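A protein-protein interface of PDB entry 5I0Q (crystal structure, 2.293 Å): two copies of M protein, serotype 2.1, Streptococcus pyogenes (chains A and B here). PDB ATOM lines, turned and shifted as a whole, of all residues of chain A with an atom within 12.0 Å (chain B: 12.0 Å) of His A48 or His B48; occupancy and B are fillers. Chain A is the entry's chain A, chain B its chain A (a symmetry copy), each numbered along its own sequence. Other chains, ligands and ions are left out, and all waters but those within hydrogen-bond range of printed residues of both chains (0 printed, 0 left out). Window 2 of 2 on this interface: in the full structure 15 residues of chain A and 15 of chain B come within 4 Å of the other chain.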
ATOM      1  N   GLU A  39     -34.889  -1.047  11.404  1.00  0.00           N
ATOM      2  CA  GLU A  39     -34.607   0.358  11.097  1.00  0.00           C
ATOM      3  C   GLU A  39     -33.267   0.781  11.687  1.00  0.00           C
ATOM      4  O   GLU A  39     -32.458   1.414  11.012  1.00  0.00           O
ATOM      5  CB  GLU A  39     -35.713   1.278  11.622  1.00  0.00           C
ATOM      6  CG  GLU A  39     -37.094   0.992  11.055  1.00  0.00           C
ATOM      7  CD  GLU A  39     -37.207   1.309   9.573  1.00  0.00           C
ATOM      8  OE1 GLU A  39     -36.753   2.399   9.172  1.00  0.00           O
ATOM      9  OE2 GLU A  39     -37.753   0.471   8.815  1.00  0.00           O
ATOM     10  N   LYS A  40     -33.039   0.432  12.950  1.00  0.00           N
ATOM     11  CA  LYS A  40     -31.771   0.723  13.612  1.00  0.00           C
ATOM     12  C   LYS A  40     -30.603   0.117  12.844  1.00  0.00           C
ATOM     13  O   LYS A  40     -29.556   0.748  12.675  1.00  0.00           O
ATOM     14  CB  LYS A  40     -31.782   0.197  15.045  1.00  0.00           C
ATOM     15  CG  LYS A  40     -31.954   1.262  16.115  1.00  0.00           C
ATOM     16  CD  LYS A  40     -30.629   1.572  16.795  1.00  0.00           C
ATOM     17  CE  LYS A  40     -30.130   0.391  17.618  1.00  0.00           C
ATOM     18  NZ  LYS A  40     -30.461   0.513  19.071  1.00  0.00           N
ATOM     19  N   LEU A  41     -30.802  -1.107  12.371  1.00  0.00           N
ATOM     20  CA  LEU A  41     -29.757  -1.861  11.690  1.00  0.00           C
ATOM     21  C   LEU A  41     -29.294  -1.171  10.400  1.00  0.00           C
ATOM     22  O   LEU A  41     -28.094  -1.022  10.177  1.00  0.00           O
ATOM     23  CB  LEU A  41     -30.253  -3.283  11.407  1.00  0.00           C
ATOM     24  CG  LEU A  41     -29.310  -4.407  10.971  1.00  0.00           C
ATOM     25  CD1 LEU A  41     -29.245  -4.510   9.469  1.00  0.00           C
ATOM     26  CD2 LEU A  41     -27.917  -4.210  11.535  1.00  0.00           C
ATOM     27  N   ASP A  42     -30.217  -0.726   9.554  1.00  0.00           N
ATOM     28  CA  ASP A  42     -29.767  -0.121   8.299  1.00  0.00           C
ATOM     29  C   ASP A  42     -29.423   1.372   8.458  1.00  0.00           C
ATOM     30  O   ASP A  42     -28.624   1.901   7.695  1.00  0.00           O
ATOM     31  CB  ASP A  42     -30.793  -0.343   7.168  1.00  0.00           C
ATOM     32  CG  ASP A  42     -32.132   0.321   7.422  1.00  0.00           C
ATOM     33  OD1 ASP A  42     -32.251   1.150   8.342  1.00  0.00           O
ATOM     34  OD2 ASP A  42     -33.075   0.027   6.665  1.00  0.00           O
ATOM     35  N   LYS A  43     -29.997   2.036   9.457  1.00  0.00           N
ATOM     36  CA  LYS A  43     -29.630   3.420   9.758  1.00  0.00           C
ATOM     37  C   LYS A  43     -28.200   3.491  10.313  1.00  0.00           C
ATOM     38  O   LYS A  43     -27.486   4.475  10.106  1.00  0.00           O
ATOM     39  CB  LYS A  43     -30.628   4.041  10.743  1.00  0.00           C
ATOM     40  CG  LYS A  43     -29.999   4.692  11.978  1.00  0.00           C
ATOM     41  CD  LYS A  43     -29.825   6.199  11.819  1.00  0.00           C
ATOM     42  CE  LYS A  43     -30.975   6.966  12.465  1.00  0.00           C
ATOM     43  NZ  LYS A  43     -32.314   6.543  11.952  1.00  0.00           N
ATOM     44  N   VAL A  44     -27.794   2.443  11.023  1.00  0.00           N
ATOM     45  CA  VAL A  44     -26.417   2.308  11.485  1.00  0.00           C
ATOM     46  C   VAL A  44     -25.532   1.869  10.324  1.00  0.00           C
ATOM     47  O   VAL A  44     -24.399   2.327  10.181  1.00  0.00           O
ATOM     48  CB  VAL A  44     -26.310   1.291  12.647  1.00  0.00           C
ATOM     49  CG1 VAL A  44     -24.936   0.648  12.693  1.00  0.00           C
ATOM     50  CG2 VAL A  44     -26.650   1.954  13.978  1.00  0.00           C
ATOM     51  N   GLU A  45     -26.071   0.995   9.479  1.00  0.00           N
ATOM     52  CA  GLU A  45     -25.319   0.427   8.366  1.00  0.00           C
ATOM     53  C   GLU A  45     -25.159   1.415   7.213  1.00  0.00           C
ATOM     54  O   GLU A  45     -24.201   1.328   6.442  1.00  0.00           O
ATOM     55  CB  GLU A  45     -26.002  -0.847   7.871  1.00  0.00           C
ATOM     56  CG  GLU A  45     -25.050  -1.942   7.437  1.00  0.00           C
ATOM     57  CD  GLU A  45     -25.736  -3.291   7.333  1.00  0.00           C
ATOM     58  OE1 GLU A  45     -26.979  -3.339   7.454  1.00  0.00           O
ATOM     59  OE2 GLU A  45     -25.031  -4.303   7.138  1.00  0.00           O
ATOM     60  N   GLU A  46     -26.097   2.349   7.093  1.00  0.00           N
ATOM     61  CA  GLU A  46     -26.009   3.376   6.062  1.00  0.00           C
ATOM     62  C   GLU A  46     -24.920   4.386   6.393  1.00  0.00           C
ATOM     63  O   GLU A  46     -23.989   4.586   5.611  1.00  0.00           O
ATOM     64  CB  GLU A  46     -27.350   4.100   5.883  1.00  0.00           C
ATOM     65  CG  GLU A  46     -28.358   3.386   4.979  1.00  0.00           C
ATOM     66  CD  GLU A  46     -28.076   3.581   3.496  1.00  0.00           C
ATOM     67  OE1 GLU A  46     -29.032   3.860   2.739  1.00  0.00           O
ATOM     68  OE2 GLU A  46     -26.905   3.452   3.082  1.00  0.00           O
ATOM     69  N   GLU A  47     -25.030   5.018   7.557  1.00  0.00           N
ATOM     70  CA  GLU A  47     -24.122   6.100   7.922  1.00  0.00           C
ATOM     71  C   GLU A  47     -22.725   5.602   8.285  1.00  0.00           C
ATOM     72  O   GLU A  47     -21.802   6.399   8.457  1.00  0.00           O
ATOM     73  CB  GLU A  47     -24.699   6.913   9.083  1.00  0.00           C
ATOM     74  CG  GLU A  47     -24.697   6.190  10.414  1.00  0.00           C
ATOM     75  CD  GLU A  47     -25.185   7.072  11.546  1.00  0.00           C
ATOM     76  OE1 GLU A  47     -25.537   8.238  11.271  1.00  0.00           O
ATOM     77  OE2 GLU A  47     -25.217   6.601  12.704  1.00  0.00           O
ATOM     78  N   HIS A  48     -22.568   4.287   8.402  1.00  0.00           N
ATOM     79  CA  HIS A  48     -21.252   3.699   8.624  1.00  0.00           C
ATOM     80  C   HIS A  48     -20.673   3.234   7.290  1.00  0.00           C
ATOM     81  O   HIS A  48     -19.710   2.466   7.248  1.00  0.00           O
ATOM     82  CB  HIS A  48     -21.329   2.533   9.616  1.00  0.00           C
ATOM     83  CG  HIS A  48     -20.248   2.542  10.652  1.00  0.00           C
ATOM     84  ND1 HIS A  48     -19.307   3.547  10.742  1.00  0.00           N
ATOM     85  CD2 HIS A  48     -19.960   1.669  11.648  1.00  0.00           C
ATOM     86  CE1 HIS A  48     -18.487   3.292  11.746  1.00  0.00           C
ATOM     87  NE2 HIS A  48     -18.860   2.159  12.312  1.00  0.00           N
ATOM     88  N   LYS A  49     -21.272   3.710   6.201  1.00  0.00           N
ATOM     89  CA  LYS A  49     -20.835   3.360   4.854  1.00  0.00           C
ATOM     90  C   LYS A  49     -20.967   4.544   3.899  1.00  0.00           C
ATOM     91  O   LYS A  49     -19.977   5.190   3.551  1.00  0.00           O
ATOM     92  CB  LYS A  49     -21.635   2.171   4.325  1.00  0.00           C
ATOM     93  CG  LYS A  49     -21.299   1.786   2.896  1.00  0.00           C
ATOM     94  CD  LYS A  49     -22.197   0.666   2.404  1.00  0.00           C
ATOM     95  CE  LYS A  49     -21.880   0.302   0.963  1.00  0.00           C
ATOM     96  NZ  LYS A  49     -22.848  -0.692   0.416  1.00  0.00           N
ATOM     97  N   GLU B  39     -27.605  -9.807  17.730  1.00  0.00           N
ATOM     98  CA  GLU B  39     -26.290 -10.352  17.387  1.00  0.00           C
ATOM     99  C   GLU B  39     -25.803  -9.794  16.054  1.00  0.00           C
ATOM    100  O   GLU B  39     -24.654  -9.374  15.933  1.00  0.00           O
ATOM    101  CB  GLU B  39     -26.316 -11.882  17.322  1.00  0.00           C
ATOM    102  CG  GLU B  39     -26.728 -12.560  18.619  1.00  0.00           C
ATOM    103  CD  GLU B  39     -25.708 -12.388  19.732  1.00  0.00           C
ATOM    104  OE1 GLU B  39     -24.507 -12.590  19.459  1.00  0.00           O
ATOM    105  OE2 GLU B  39     -26.108 -12.061  20.875  1.00  0.00           O
ATOM    106  N   LYS B  40     -26.682  -9.795  15.057  1.00  0.00           N
ATOM    107  CA  LYS B  40     -26.361  -9.232  13.748  1.00  0.00           C
ATOM    108  C   LYS B  40     -25.943  -7.773  13.870  1.00  0.00           C
ATOM    109  O   LYS B  40     -24.989  -7.328  13.225  1.00  0.00           O
ATOM    110  CB  LYS B  40     -27.557  -9.354  12.806  1.00  0.00           C
ATOM    111  CG  LYS B  40     -27.432 -10.445  11.755  1.00  0.00           C
ATOM    112  CD  LYS B  40     -27.086  -9.856  10.395  1.00  0.00           C
ATOM    113  CE  LYS B  40     -28.234  -9.025   9.835  1.00  0.00           C
ATOM    114  NZ  LYS B  40     -29.079  -9.779   8.861  1.00  0.00           N
ATOM    115  N   LEU B  41     -26.658  -7.039  14.715  1.00  0.00           N
ATOM    116  CA  LEU B  41     -26.443  -5.609  14.883  1.00  0.00           C
ATOM    117  C   LEU B  41     -25.038  -5.294  15.414  1.00  0.00           C
ATOM    118  O   LEU B  41     -24.352  -4.429  14.870  1.00  0.00           O
ATOM    119  CB  LEU B  41     -27.521  -5.033  15.807  1.00  0.00           C
ATOM    120  CG  LEU B  41     -27.756  -3.528  15.954  1.00  0.00           C
ATOM    121  CD1 LEU B  41     -26.967  -2.966  17.110  1.00  0.00           C
ATOM    122  CD2 LEU B  41     -27.403  -2.786  14.680  1.00  0.00           C
ATOM    123  N   ASP B  42     -24.581  -5.990  16.450  1.00  0.00           N
ATOM    124  CA  ASP B  42     -23.263  -5.645  16.984  1.00  0.00           C
ATOM    125  C   ASP B  42     -22.120  -6.336  16.220  1.00  0.00           C
ATOM    126  O   ASP B  42     -21.001  -5.834  16.203  1.00  0.00           O
ATOM    127  CB  ASP B  42     -23.179  -5.928  18.499  1.00  0.00           C
ATOM    128  CG  ASP B  42     -23.332  -7.395  18.852  1.00  0.00           C
ATOM    129  OD1 ASP B  42     -23.279  -8.259  17.959  1.00  0.00           O
ATOM    130  OD2 ASP B  42     -23.480  -7.686  20.052  1.00  0.00           O
ATOM    131  N   LYS B  43     -22.402  -7.462  15.570  1.00  0.00           N
ATOM    132  CA  LYS B  43     -21.409  -8.114  14.715  1.00  0.00           C
ATOM    133  C   LYS B  43     -21.132  -7.268  13.467  1.00  0.00           C
ATOM    134  O   LYS B  43     -20.021  -7.269  12.931  1.00  0.00           O
ATOM    135  CB  LYS B  43     -21.876  -9.523  14.327  1.00  0.00           C
ATOM    136  CG  LYS B  43     -21.850  -9.822  12.824  1.00  0.00           C
ATOM    137  CD  LYS B  43     -20.580 -10.553  12.398  1.00  0.00           C
ATOM    138  CE  LYS B  43     -20.806 -12.060  12.312  1.00  0.00           C
ATOM    139  NZ  LYS B  43     -21.334 -12.640  13.584  1.00  0.00           N
ATOM    140  N   VAL B  44     -22.152  -6.549  13.006  1.00  0.00           N
ATOM    141  CA  VAL B  44     -21.994  -5.589  11.920  1.00  0.00           C
ATOM    142  C   VAL B  44     -21.337  -4.321  12.454  1.00  0.00           C
ATOM    143  O   VAL B  44     -20.494  -3.717  11.792  1.00  0.00           O
ATOM    144  CB  VAL B  44     -23.355  -5.246  11.267  1.00  0.00           C
ATOM    145  CG1 VAL B  44     -23.341  -3.858  10.657  1.00  0.00           C
ATOM    146  CG2 VAL B  44     -23.737  -6.297  10.231  1.00  0.00           C
ATOM    147  N   GLU B  45     -21.712  -3.938  13.670  1.00  0.00           N
ATOM    148  CA  GLU B  45     -21.228  -2.706  14.280  1.00  0.00           C
ATOM    149  C   GLU B  45     -19.793  -2.835  14.784  1.00  0.00           C
ATOM    150  O   GLU B  45     -19.067  -1.843  14.871  1.00  0.00           O
ATOM    151  CB  GLU B  45     -22.149  -2.295  15.428  1.00  0.00           C
ATOM    152  CG  GLU B  45     -22.359  -0.800  15.560  1.00  0.00           C
ATOM    153  CD  GLU B  45     -23.555  -0.464  16.429  1.00  0.00           C
ATOM    154  OE1 GLU B  45     -24.125  -1.390  17.046  1.00  0.00           O
ATOM    155  OE2 GLU B  45     -23.930   0.727  16.490  1.00  0.00           O
ATOM    156  N   GLU B  46     -19.387  -4.056  15.121  1.00  0.00           N
ATOM    157  CA  GLU B  46     -18.017  -4.300  15.559  1.00  0.00           C
ATOM    158  C   GLU B  46     -17.047  -4.203  14.390  1.00  0.00           C
ATOM    159  O   GLU B  46     -16.114  -3.398  14.414  1.00  0.00           O
ATOM    160  CB  GLU B  46     -17.885  -5.673  16.230  1.00  0.00           C
ATOM    161  CG  GLU B  46     -18.284  -5.716  17.707  1.00  0.00           C
ATOM    162  CD  GLU B  46     -17.206  -5.179  18.635  1.00  0.00           C
ATOM    163  OE1 GLU B  46     -16.934  -5.827  19.671  1.00  0.00           O
ATOM    164  OE2 GLU B  46     -16.630  -4.111  18.339  1.00  0.00           O
ATOM    165  N   GLU B  47     -17.273  -5.014  13.362  1.00  0.00           N
ATOM    166  CA  GLU B  47     -16.337  -5.105  12.247  1.00  0.00           C
ATOM    167  C   GLU B  47     -16.384  -3.880  11.334  1.00  0.00           C
ATOM    168  O   GLU B  47     -15.545  -3.731  10.447  1.00  0.00           O
ATOM    169  CB  GLU B  47     -16.601  -6.369  11.429  1.00  0.00           C
ATOM    170  CG  GLU B  47     -17.879  -6.333  10.616  1.00  0.00           C
ATOM    171  CD  GLU B  47     -18.044  -7.566   9.751  1.00  0.00           C
ATOM    172  OE1 GLU B  47     -17.159  -8.447   9.808  1.00  0.00           O
ATOM    173  OE2 GLU B  47     -19.052  -7.654   9.016  1.00  0.00           O
ATOM    174  N   HIS B  48     -17.363  -3.007  11.552  1.00  0.00           N
ATOM    175  CA  HIS B  48     -17.429  -1.747  10.821  1.00  0.00           C
ATOM    176  C   HIS B  48     -16.809  -0.637  11.668  1.00  0.00           C
ATOM    177  O   HIS B  48     -16.992   0.549  11.394  1.00  0.00           O
ATOM    178  CB  HIS B  48     -18.875  -1.401  10.450  1.00  0.00           C
ATOM    179  CG  HIS B  48     -19.042  -0.918   9.042  1.00  0.00           C
ATOM    180  ND1 HIS B  48     -17.997  -0.855   8.144  1.00  0.00           N
ATOM    181  CD2 HIS B  48     -20.137  -0.479   8.374  1.00  0.00           C
ATOM    182  CE1 HIS B  48     -18.439  -0.396   6.986  1.00  0.00           C
ATOM    183  NE2 HIS B  48     -19.733  -0.161   7.099  1.00  0.00           N
ATOM    184  N   LYS B  49     -16.073  -1.040  12.701  1.00  0.00           N
ATOM    185  CA  LYS B  49     -15.414  -0.101  13.603  1.00  0.00           C
ATOM    186  C   LYS B  49     -14.054  -0.625  14.059  1.00  0.00           C
ATOM    187  O   LYS B  49     -13.011  -0.177  13.579  1.00  0.00           O
ATOM    188  CB  LYS B  49     -16.297   0.183  14.817  1.00  0.00           C
ATOM    189  CG  LYS B  49     -15.657   1.093  15.849  1.00  0.00           C
ATOM    190  CD  LYS B  49     -16.547   1.251  17.067  1.00  0.00           C
ATOM    191  CE  LYS B  49     -15.890   2.138  18.113  1.00  0.00           C
ATOM    192  NZ  LYS B  49     -16.683   2.187  19.376  1.00  0.00           N
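O of His A48 lies within hydrogen-bond range of NE2 of His B48 (2.6 Å).
CD2 of Leu B41 touches CD2 of Leu A41, 3.5 Å away. Val A44 touches Glu B45. Glu A45 touches Val B44.
Printed residues of chain B within 4 Å of Leu A41: Leu B41. Asp A42 touches none of the printed residues of chain B. Of the printed residues of chain B, Glu A45 touches Val B44 (3.9 Å). No residue of chain B comes within 4 Å of Glu A47. His A48 touches one residue of chain B. Lys A49 touches none of the printed residues of chain B. Printed residues of chain A within 4 Å of Leu B41: Leu A41. Val B44 touches one residue of chain A. Glu B45 touches just one residue of chain A: Val A44 (3.9 Å). Of chain A, only His A48 (2.6 Å) comes within 4 Å of His B48. No residue of chain A comes within 4 Å of Lys B49. The nearest residue of chain B that does not touch His A48 is Lys B49 (4.1 Å).
Hydrophobic or aromatic side chains of chain B within 4 Å of the printed part of chain A: Leu B41, Val B44 and His B48. Among the printed residues, 4 pairs touch across the chains.
Leu A41 touches its own counterpart, Leu B41. Val A44 touches Glu B45, and with the chains exchanged Glu A45 touches Val B44. His A48 touches its own counterpart, His B48. Positions printed for both chains: 39, 40, 41, 42, 43, 44, 45, 46, 47, 48 and 49.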
